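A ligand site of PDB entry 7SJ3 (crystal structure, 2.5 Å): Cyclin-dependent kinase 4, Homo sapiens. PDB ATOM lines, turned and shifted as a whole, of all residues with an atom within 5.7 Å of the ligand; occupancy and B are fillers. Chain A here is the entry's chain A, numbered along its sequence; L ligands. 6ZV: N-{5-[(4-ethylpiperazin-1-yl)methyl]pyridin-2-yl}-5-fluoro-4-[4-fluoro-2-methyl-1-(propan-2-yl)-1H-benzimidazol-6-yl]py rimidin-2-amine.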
ATOM      1  N   GLU A  11      29.393   3.083  20.630  1.00  0.00           N
ATOM      2  CA  GLU A  11      29.632   3.965  21.767  1.00  0.00           C
ATOM      3  C   GLU A  11      28.434   4.878  21.935  1.00  0.00           C
ATOM      4  O   GLU A  11      28.028   5.545  20.991  1.00  0.00           O
ATOM      5  CB  GLU A  11      30.889   4.803  21.549  1.00  0.00           C
ATOM      6  CG  GLU A  11      32.116   4.362  22.303  1.00  0.00           C
ATOM      7  CD  GLU A  11      33.324   5.218  21.976  1.00  0.00           C
ATOM      8  OE1 GLU A  11      33.179   6.212  21.225  1.00  0.00           O
ATOM      9  OE2 GLU A  11      34.439   4.894  22.445  1.00  0.00           O
ATOM     10  N   ILE A  12      27.890   4.939  23.153  1.00  0.00           N
ATOM     11  CA  ILE A  12      26.672   5.720  23.355  1.00  0.00           C
ATOM     12  C   ILE A  12      26.897   6.846  24.341  1.00  0.00           C
ATOM     13  O   ILE A  12      25.975   7.620  24.612  1.00  0.00           O
ATOM     14  CB  ILE A  12      25.496   4.828  23.807  1.00  0.00           C
ATOM     15  CG1 ILE A  12      25.846   4.011  25.048  1.00  0.00           C
ATOM     16  CG2 ILE A  12      25.070   3.891  22.685  1.00  0.00           C
ATOM     17  CD1 ILE A  12      24.710   3.090  25.487  1.00  0.00           C
ATOM     18  N   GLY A  13      28.097   6.964  24.891  1.00  0.00           N
ATOM     19  CA  GLY A  13      28.456   8.055  25.762  1.00  0.00           C
ATOM     20  C   GLY A  13      29.883   7.955  26.276  1.00  0.00           C
ATOM     21  O   GLY A  13      30.390   6.848  26.476  1.00  0.00           O
ATOM     22  N   TYR A  17      33.828   9.390  33.909  1.00  0.00           N
ATOM     23  CA  TYR A  17      33.502   8.138  34.568  1.00  0.00           C
ATOM     24  C   TYR A  17      33.901   6.934  33.712  1.00  0.00           C
ATOM     25  O   TYR A  17      34.078   5.834  34.258  1.00  0.00           O
ATOM     26  CB  TYR A  17      31.984   7.993  34.795  1.00  0.00           C
ATOM     27  CG  TYR A  17      31.170   8.133  33.515  1.00  0.00           C
ATOM     28  CD1 TYR A  17      30.903   9.374  32.949  1.00  0.00           C
ATOM     29  CD2 TYR A  17      30.814   7.014  32.778  1.00  0.00           C
ATOM     30  CE1 TYR A  17      30.187   9.482  31.761  1.00  0.00           C
ATOM     31  CE2 TYR A  17      30.127   7.105  31.576  1.00  0.00           C
ATOM     32  CZ  TYR A  17      29.827   8.351  31.065  1.00  0.00           C
ATOM     33  OH  TYR A  17      29.122   8.437  29.874  1.00  0.00           O
ATOM     34  N   VAL A  20      30.257   4.290  27.970  1.00  0.00           N
ATOM     35  CA  VAL A  20      29.063   3.451  27.955  1.00  0.00           C
ATOM     36  C   VAL A  20      28.925   2.905  26.534  1.00  0.00           C
ATOM     37  O   VAL A  20      29.109   3.653  25.560  1.00  0.00           O
ATOM     38  CB  VAL A  20      27.791   4.206  28.373  1.00  0.00           C
ATOM     39  CG1 VAL A  20      26.628   3.236  28.511  1.00  0.00           C
ATOM     40  CG2 VAL A  20      28.003   4.940  29.676  1.00  0.00           C
ATOM     41  N   ALA A  33      23.748  -2.937  27.697  1.00  0.00           N
ATOM     42  CA  ALA A  33      24.598  -1.758  27.747  1.00  0.00           C
ATOM     43  C   ALA A  33      25.749  -2.032  28.702  1.00  0.00           C
ATOM     44  O   ALA A  33      25.562  -2.649  29.751  1.00  0.00           O
ATOM     45  CB  ALA A  33      23.825  -0.511  28.186  1.00  0.00           C
ATOM     46  N   LYS A  35      28.960  -0.226  30.766  1.00  0.00           N
ATOM     47  CA  LYS A  35      29.582   0.976  31.290  1.00  0.00           C
ATOM     48  C   LYS A  35      30.936   0.567  31.829  1.00  0.00           C
ATOM     49  O   LYS A  35      31.019  -0.181  32.823  1.00  0.00           O
ATOM     50  CB  LYS A  35      28.728   1.629  32.375  1.00  0.00           C
ATOM     51  CG  LYS A  35      29.306   2.932  32.906  1.00  0.00           C
ATOM     52  CD  LYS A  35      28.300   3.619  33.817  1.00  0.00           C
ATOM     53  CE  LYS A  35      28.852   4.881  34.424  1.00  0.00           C
ATOM     54  NZ  LYS A  35      27.749   5.658  35.079  1.00  0.00           N
ATOM     55  N   GLU A  56      27.921   4.025  42.835  1.00  0.00           N
ATOM     56  CA  GLU A  56      26.888   3.732  41.840  1.00  0.00           C
ATOM     57  C   GLU A  56      26.474   2.276  41.902  1.00  0.00           C
ATOM     58  O   GLU A  56      25.284   1.947  41.917  1.00  0.00           O
ATOM     59  CB  GLU A  56      27.382   4.130  40.437  1.00  0.00           C
ATOM     60  CG  GLU A  56      26.510   3.576  39.301  1.00  0.00           C
ATOM     61  CD  GLU A  56      26.915   4.112  37.946  1.00  0.00           C
ATOM     62  OE1 GLU A  56      28.108   4.062  37.602  1.00  0.00           O
ATOM     63  OE2 GLU A  56      26.015   4.572  37.211  1.00  0.00           O
ATOM     64  N   VAL A  72      16.773   1.778  35.468  1.00  0.00           N
ATOM     65  CA  VAL A  72      17.552   0.811  34.708  1.00  0.00           C
ATOM     66  C   VAL A  72      17.955  -0.335  35.628  1.00  0.00           C
ATOM     67  O   VAL A  72      18.185  -0.156  36.836  1.00  0.00           O
ATOM     68  CB  VAL A  72      18.801   1.454  34.080  1.00  0.00           C
ATOM     69  CG1 VAL A  72      18.388   2.531  33.078  1.00  0.00           C
ATOM     70  CG2 VAL A  72      19.703   2.047  35.163  1.00  0.00           C
ATOM     71  N   LEU A  91      30.176  -2.551  34.182  1.00  0.00           N
ATOM     72  CA  LEU A  91      28.796  -2.742  34.625  1.00  0.00           C
ATOM     73  C   LEU A  91      27.938  -3.127  33.430  1.00  0.00           C
ATOM     74  O   LEU A  91      28.069  -2.541  32.340  1.00  0.00           O
ATOM     75  CB  LEU A  91      28.249  -1.461  35.273  1.00  0.00           C
ATOM     76  CG  LEU A  91      29.076  -0.535  36.173  1.00  0.00           C
ATOM     77  CD1 LEU A  91      28.168   0.267  37.096  1.00  0.00           C
ATOM     78  CD2 LEU A  91      30.058  -1.320  37.012  1.00  0.00           C
ATOM     79  N   PHE A  93      24.099  -3.471  32.004  1.00  0.00           N
ATOM     80  CA  PHE A  93      22.724  -3.015  32.146  1.00  0.00           C
ATOM     81  C   PHE A  93      21.882  -3.651  31.051  1.00  0.00           C
ATOM     82  O   PHE A  93      22.359  -3.881  29.938  1.00  0.00           O
ATOM     83  CB  PHE A  93      22.603  -1.497  32.057  1.00  0.00           C
ATOM     84  CG  PHE A  93      23.252  -0.744  33.184  1.00  0.00           C
ATOM     85  CD1 PHE A  93      24.570  -0.326  33.102  1.00  0.00           C
ATOM     86  CD2 PHE A  93      22.521  -0.421  34.317  1.00  0.00           C
ATOM     87  CE1 PHE A  93      25.154   0.388  34.138  1.00  0.00           C
ATOM     88  CE2 PHE A  93      23.096   0.294  35.354  1.00  0.00           C
ATOM     89  CZ  PHE A  93      24.413   0.702  35.267  1.00  0.00           C
ATOM     90  N   GLU A  94      20.605  -3.899  31.361  1.00  0.00           N
ATOM     91  CA  GLU A  94      19.634  -4.165  30.313  1.00  0.00           C
ATOM     92  C   GLU A  94      19.541  -2.959  29.381  1.00  0.00           C
ATOM     93  O   GLU A  94      19.543  -1.806  29.819  1.00  0.00           O
ATOM     94  CB  GLU A  94      18.253  -4.493  30.899  1.00  0.00           C
ATOM     95  CG  GLU A  94      17.528  -3.322  31.553  1.00  0.00           C
ATOM     96  CD  GLU A  94      16.076  -3.615  31.835  1.00  0.00           C
ATOM     97  OE1 GLU A  94      15.668  -4.799  31.758  1.00  0.00           O
ATOM     98  OE2 GLU A  94      15.335  -2.652  32.144  1.00  0.00           O
ATOM     99  N   HIS A  95      19.552  -3.232  28.074  1.00  0.00           N
ATOM    100  CA  HIS A  95      19.651  -2.178  27.091  1.00  0.00           C
ATOM    101  C   HIS A  95      18.323  -1.437  26.919  1.00  0.00           C
ATOM    102  O   HIS A  95      17.258  -2.050  26.879  1.00  0.00           O
ATOM    103  CB  HIS A  95      20.084  -2.757  25.743  1.00  0.00           C
ATOM    104  CG  HIS A  95      20.156  -1.743  24.648  1.00  0.00           C
ATOM    105  ND1 HIS A  95      21.007  -0.657  24.680  1.00  0.00           N
ATOM    106  CD2 HIS A  95      19.446  -1.615  23.505  1.00  0.00           C
ATOM    107  CE1 HIS A  95      20.830   0.082  23.607  1.00  0.00           C
ATOM    108  NE2 HIS A  95      19.881  -0.480  22.864  1.00  0.00           N
ATOM    109  N   VAL A  96      18.421  -0.111  26.809  1.00  0.00           N
ATOM    110  CA  VAL A  96      17.286   0.752  26.484  1.00  0.00           C
ATOM    111  C   VAL A  96      17.630   1.449  25.173  1.00  0.00           C
ATOM    112  O   VAL A  96      18.773   1.841  24.946  1.00  0.00           O
ATOM    113  CB  VAL A  96      17.000   1.768  27.609  1.00  0.00           C
ATOM    114  CG1 VAL A  96      15.681   2.473  27.357  1.00  0.00           C
ATOM    115  CG2 VAL A  96      16.924   1.065  28.948  1.00  0.00           C
ATOM    116  N   ASP A  97      16.611   1.625  24.323  1.00  0.00           N
ATOM    117  CA  ASP A  97      16.886   2.009  22.942  1.00  0.00           C
ATOM    118  C   ASP A  97      17.289   3.468  22.814  1.00  0.00           C
ATOM    119  O   ASP A  97      18.048   3.812  21.900  1.00  0.00           O
ATOM    120  CB  ASP A  97      15.678   1.705  22.045  1.00  0.00           C
ATOM    121  CG  ASP A  97      15.847   0.419  21.255  1.00  0.00           C
ATOM    122  OD1 ASP A  97      16.925  -0.202  21.355  1.00  0.00           O
ATOM    123  OD2 ASP A  97      14.905   0.026  20.537  1.00  0.00           O
ATOM    124  N   GLN A  98      16.842   4.327  23.718  1.00  0.00           N
ATOM    125  CA  GLN A  98      17.031   5.751  23.507  1.00  0.00           C
ATOM    126  C   GLN A  98      16.870   6.493  24.826  1.00  0.00           C
ATOM    127  O   GLN A  98      16.440   5.932  25.835  1.00  0.00           O
ATOM    128  CB  GLN A  98      16.029   6.276  22.478  1.00  0.00           C
ATOM    129  CG  GLN A  98      14.625   6.396  23.042  1.00  0.00           C
ATOM    130  CD  GLN A  98      13.546   6.112  22.015  1.00  0.00           C
ATOM    131  OE1 GLN A  98      13.490   6.752  20.967  1.00  0.00           O
ATOM    132  NE2 GLN A  98      12.684   5.140  22.316  1.00  0.00           N
ATOM    133  N   ASP A  99      17.194   7.778  24.790  1.00  0.00           N
ATOM    134  CA  ASP A  99      16.971   8.685  25.899  1.00  0.00           C
ATOM    135  C   ASP A  99      15.765   9.581  25.583  1.00  0.00           C
ATOM    136  O   ASP A  99      15.151   9.475  24.523  1.00  0.00           O
ATOM    137  CB  ASP A  99      18.222   9.512  26.199  1.00  0.00           C
ATOM    138  CG  ASP A  99      18.692  10.351  25.014  1.00  0.00           C
ATOM    139  OD1 ASP A  99      17.965  10.433  23.998  1.00  0.00           O
ATOM    140  OD2 ASP A  99      19.800  10.919  25.113  1.00  0.00           O
ATOM    141  N   THR A 102      15.894  11.722  22.217  1.00  0.00           N
ATOM    142  CA  THR A 102      15.614  10.904  21.031  1.00  0.00           C
ATOM    143  C   THR A 102      14.143  10.526  20.932  1.00  0.00           C
ATOM    144  O   THR A 102      13.593  10.416  19.834  1.00  0.00           O
ATOM    145  CB  THR A 102      16.510   9.668  21.040  1.00  0.00           C
ATOM    146  OG1 THR A 102      17.879  10.091  21.149  1.00  0.00           O
ATOM    147  CG2 THR A 102      16.337   8.858  19.769  1.00  0.00           C
ATOM    148  N   GLU A 144      19.668  13.550  29.279  1.00  0.00           N
ATOM    149  CA  GLU A 144      20.547  12.464  28.852  1.00  0.00           C
ATOM    150  C   GLU A 144      20.413  11.246  29.762  1.00  0.00           C
ATOM    151  O   GLU A 144      20.621  10.115  29.308  1.00  0.00           O
ATOM    152  CB  GLU A 144      21.991  12.942  28.815  1.00  0.00           C
ATOM    153  CG  GLU A 144      22.315  13.929  27.705  1.00  0.00           C
ATOM    154  CD  GLU A 144      21.827  15.340  28.008  1.00  0.00           C
ATOM    155  OE1 GLU A 144      21.448  15.607  29.171  1.00  0.00           O
ATOM    156  OE2 GLU A 144      21.823  16.181  27.087  1.00  0.00           O
ATOM    157  N   ASN A 145      20.117  11.465  31.045  1.00  0.00           N
ATOM    158  CA  ASN A 145      19.988  10.384  32.019  1.00  0.00           C
ATOM    159  C   ASN A 145      18.578   9.832  32.124  1.00  0.00           C
ATOM    160  O   ASN A 145      18.331   8.976  32.991  1.00  0.00           O
ATOM    161  CB  ASN A 145      20.486  10.838  33.389  1.00  0.00           C
ATOM    162  CG  ASN A 145      21.965  11.162  33.399  1.00  0.00           C
ATOM    163  OD1 ASN A 145      22.711  10.725  32.513  1.00  0.00           O
ATOM    164  ND2 ASN A 145      22.396  11.937  34.381  1.00  0.00           N
ATOM    165  N   LEU A 147      16.005   7.712  30.160  1.00  0.00           N
ATOM    166  CA  LEU A 147      15.899   6.804  29.019  1.00  0.00           C
ATOM    167  C   LEU A 147      14.458   6.346  28.834  1.00  0.00           C
ATOM    168  O   LEU A 147      13.657   6.350  29.765  1.00  0.00           O
ATOM    169  CB  LEU A 147      16.812   5.596  29.202  1.00  0.00           C
ATOM    170  CG  LEU A 147      18.220   5.903  29.704  1.00  0.00           C
ATOM    171  CD1 LEU A 147      19.064   4.631  29.761  1.00  0.00           C
ATOM    172  CD2 LEU A 147      18.881   6.928  28.808  1.00  0.00           C
ATOM    173  N   ALA A 157      18.561   6.608  34.709  1.00  0.00           N
ATOM    174  CA  ALA A 157      19.899   6.075  34.565  1.00  0.00           C
ATOM    175  C   ALA A 157      20.909   7.015  35.218  1.00  0.00           C
ATOM    176  O   ALA A 157      20.581   8.115  35.677  1.00  0.00           O
ATOM    177  CB  ALA A 157      20.266   5.853  33.093  1.00  0.00           C
ATOM    178  N   ASP A 158      22.160   6.551  35.246  1.00  0.00           N
ATOM    179  CA  ASP A 158      23.327   7.272  35.746  1.00  0.00           C
ATOM    180  C   ASP A 158      23.223   7.573  37.236  1.00  0.00           C
ATOM    181  O   ASP A 158      22.764   8.658  37.630  1.00  0.00           O
ATOM    182  CB  ASP A 158      23.526   8.571  34.951  1.00  0.00           C
ATOM    183  CG  ASP A 158      24.872   9.224  35.228  1.00  0.00           C
ATOM    184  OD1 ASP A 158      25.680   8.651  35.986  1.00  0.00           O
ATOM    185  OD2 ASP A 158      25.131  10.316  34.677  1.00  0.00           O
ATOM    186  N   PHE A 159      23.664   6.639  38.081  1.00  0.00           N
ATOM    187  CA  PHE A 159      23.659   6.825  39.524  1.00  0.00           C
ATOM    188  C   PHE A 159      25.051   7.039  40.092  1.00  0.00           C
ATOM    189  O   PHE A 159      25.265   6.868  41.293  1.00  0.00           O
ATOM    190  CB  PHE A 159      22.967   5.631  40.191  1.00  0.00           C
ATOM    191  CG  PHE A 159      21.487   5.582  39.930  1.00  0.00           C
ATOM    192  CD1 PHE A 159      20.994   5.121  38.717  1.00  0.00           C
ATOM    193  CD2 PHE A 159      20.592   6.006  40.894  1.00  0.00           C
ATOM    194  CE1 PHE A 159      19.626   5.094  38.470  1.00  0.00           C
ATOM    195  CE2 PHE A 159      19.227   5.969  40.664  1.00  0.00           C
ATOM    196  CZ  PHE A 159      18.744   5.509  39.450  1.00  0.00           C
HETATM  197  C1  6ZV L   1      24.875   9.887  20.897  1.00  0.00           C
HETATM  198  C2  6ZV L   1      21.298   2.885  27.640  1.00  0.00           C
HETATM  199  C3  6ZV L   1      26.292   9.347  20.676  1.00  0.00           C
HETATM  200  C4  6ZV L   1      22.265   3.064  29.756  1.00  0.00           C
HETATM  201  C5  6ZV L   1      21.568   1.896  30.148  1.00  0.00           C
HETATM  202  C6  6ZV L   1      20.731   1.258  29.203  1.00  0.00           C
HETATM  203  N2  6ZV L   1      23.876   8.906  20.358  1.00  0.00           N
HETATM  204  C10 6ZV L   1      21.979   6.857  25.839  1.00  0.00           C
HETATM  205  C   6ZV L   1      21.863   5.615  26.418  1.00  0.00           C
HETATM  206  C17 6ZV L   1      23.516   5.098  30.188  1.00  0.00           C
HETATM  207  C21 6ZV L   1      23.665   3.301  31.812  1.00  0.00           C
HETATM  208  C12 6ZV L   1      20.782   6.027  23.946  1.00  0.00           C
HETATM  209  C16 6ZV L   1      23.173   3.839  30.614  1.00  0.00           C
HETATM  210  C11 6ZV L   1      21.438   7.100  24.577  1.00  0.00           C
HETATM  211  C19 6ZV L   1      24.902   5.310  32.209  1.00  0.00           C
HETATM  212  C18 6ZV L   1      24.387   5.834  30.996  1.00  0.00           C
HETATM  213  C20 6ZV L   1      24.525   4.032  32.608  1.00  0.00           C
HETATM  214  C8  6ZV L   1      21.194   4.595  25.714  1.00  0.00           C
HETATM  215  C23 6ZV L   1      25.750   7.302  32.030  1.00  0.00           C
HETATM  216  C31 6ZV L   1      22.064   9.648  21.882  1.00  0.00           C
HETATM  217  C35 6ZV L   1      23.493   7.814  22.571  1.00  0.00           C
HETATM  218  C32 6ZV L   1      22.491   9.469  20.411  1.00  0.00           C
HETATM  219  C34 6ZV L   1      23.941   7.600  21.100  1.00  0.00           C
HETATM  220  C25 6ZV L   1      26.532   8.535  32.298  1.00  0.00           C
HETATM  221  C27 6ZV L   1      23.240   8.391  29.615  1.00  0.00           C
HETATM  222  C28 6ZV L   1      25.326   7.545  28.504  1.00  0.00           C
HETATM  223  C14 6ZV L   1      21.560   8.451  23.943  1.00  0.00           C
HETATM  224  C26 6ZV L   1      24.734   8.090  29.804  1.00  0.00           C
HETATM  225  N   6ZV L   1      20.648   4.792  24.475  1.00  0.00           N
HETATM  226  N1  6ZV L   1      20.577   1.729  27.950  1.00  0.00           N
HETATM  227  N24 6ZV L   1      25.747   6.232  32.848  1.00  0.00           N
HETATM  228  N3  6ZV L   1      22.140   3.567  28.504  1.00  0.00           N
HETATM  229  N22 6ZV L   1      24.942   7.127  30.886  1.00  0.00           N
HETATM  230  N30 6ZV L   1      22.090   8.321  22.561  1.00  0.00           N
HETATM  231  N7  6ZV L   1      21.083   3.308  26.314  1.00  0.00           N
HETATM  232  F29 6ZV L   1      24.994   3.525  33.734  1.00  0.00           F
HETATM  233  F15 6ZV L   1      21.666   1.380  31.362  1.00  0.00           F
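The side-chain amino group (NZ) of Lys 35 is in hydrogen-bond range of a nitrogen (N24) of the ligand, 3.1 Å away.
The backbone NH (N) of Val 96 sits at hydrogen-bond distance from a nitrogen (N1) of the ligand (3.1 Å).
N7 of the ligand sits close to O of Val 96 (3.1 Å).
NZ of Lys 35 lies within salt-bridge range of OD1 of Asp 158, at 3.7 Å.
O of Lys 35 lies within hydrogen-bond range of N of Leu 91, at 2.9 Å.
O of Phe 93 lies within hydrogen-bond range of N of Ala 33, 2.8 Å away.
The side-chain carboxylate of Asp 99 is in hydrogen-bond range of the side-chain hydroxyl of Thr 102 (2.9 Å).
OD2 of Asp 158 sits at hydrogen-bond distance from ND2 of Asn 145 (3.2 Å).
O of Asn 145 sits at hydrogen-bond distance from N of Ala 157 (2.9 Å).
The side-chain carboxylate (OE2) of Glu 56 is in hydrogen-bond range of the backbone NH (N) of Phe 159, 3.2 Å away.
The side-chain carboxylate (OD1) of Asp 97 is in hydrogen-bond range of a ring nitrogen (NE2) of His 95, at 3.3 Å.
Merely in contact with the ligand: Phe 93 (3.1 Å), Glu 144 (3.2 Å), Ile 12 (3.2 Å), Asp 99 (3.2 Å), Asp 158 (3.3 Å), Glu 94 (3.3 Å), Leu 147 (3.5 Å), Tyr 17 (3.5 Å), Ala 33 (3.7 Å), Asn 145 (3.8 Å), Glu 56 (3.8 Å), Gln 98 (3.8 Å), Asp 97 (3.8 Å), Val 72 (3.9 Å) and Val 20 (3.9 Å).
Hydrophobic or aromatic side chains within 4 Å of the ligand: Ile 12, Tyr 17, Val 20, Ala 33, Val 72, Phe 93, Val 96 and Leu 147.
Within 4 Å of the ligand: Ile 12, Tyr 17, Val 20, Ala 33, Lys 35, Glu 56, Val 72, Phe 93, Glu 94, Val 96, Asp 97, Gln 98, Asp 99, Glu 144, Asn 145, Leu 147 and Asp 158.
Along chain A the residues within 4 Å of the ligand span positions 12 to 158.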
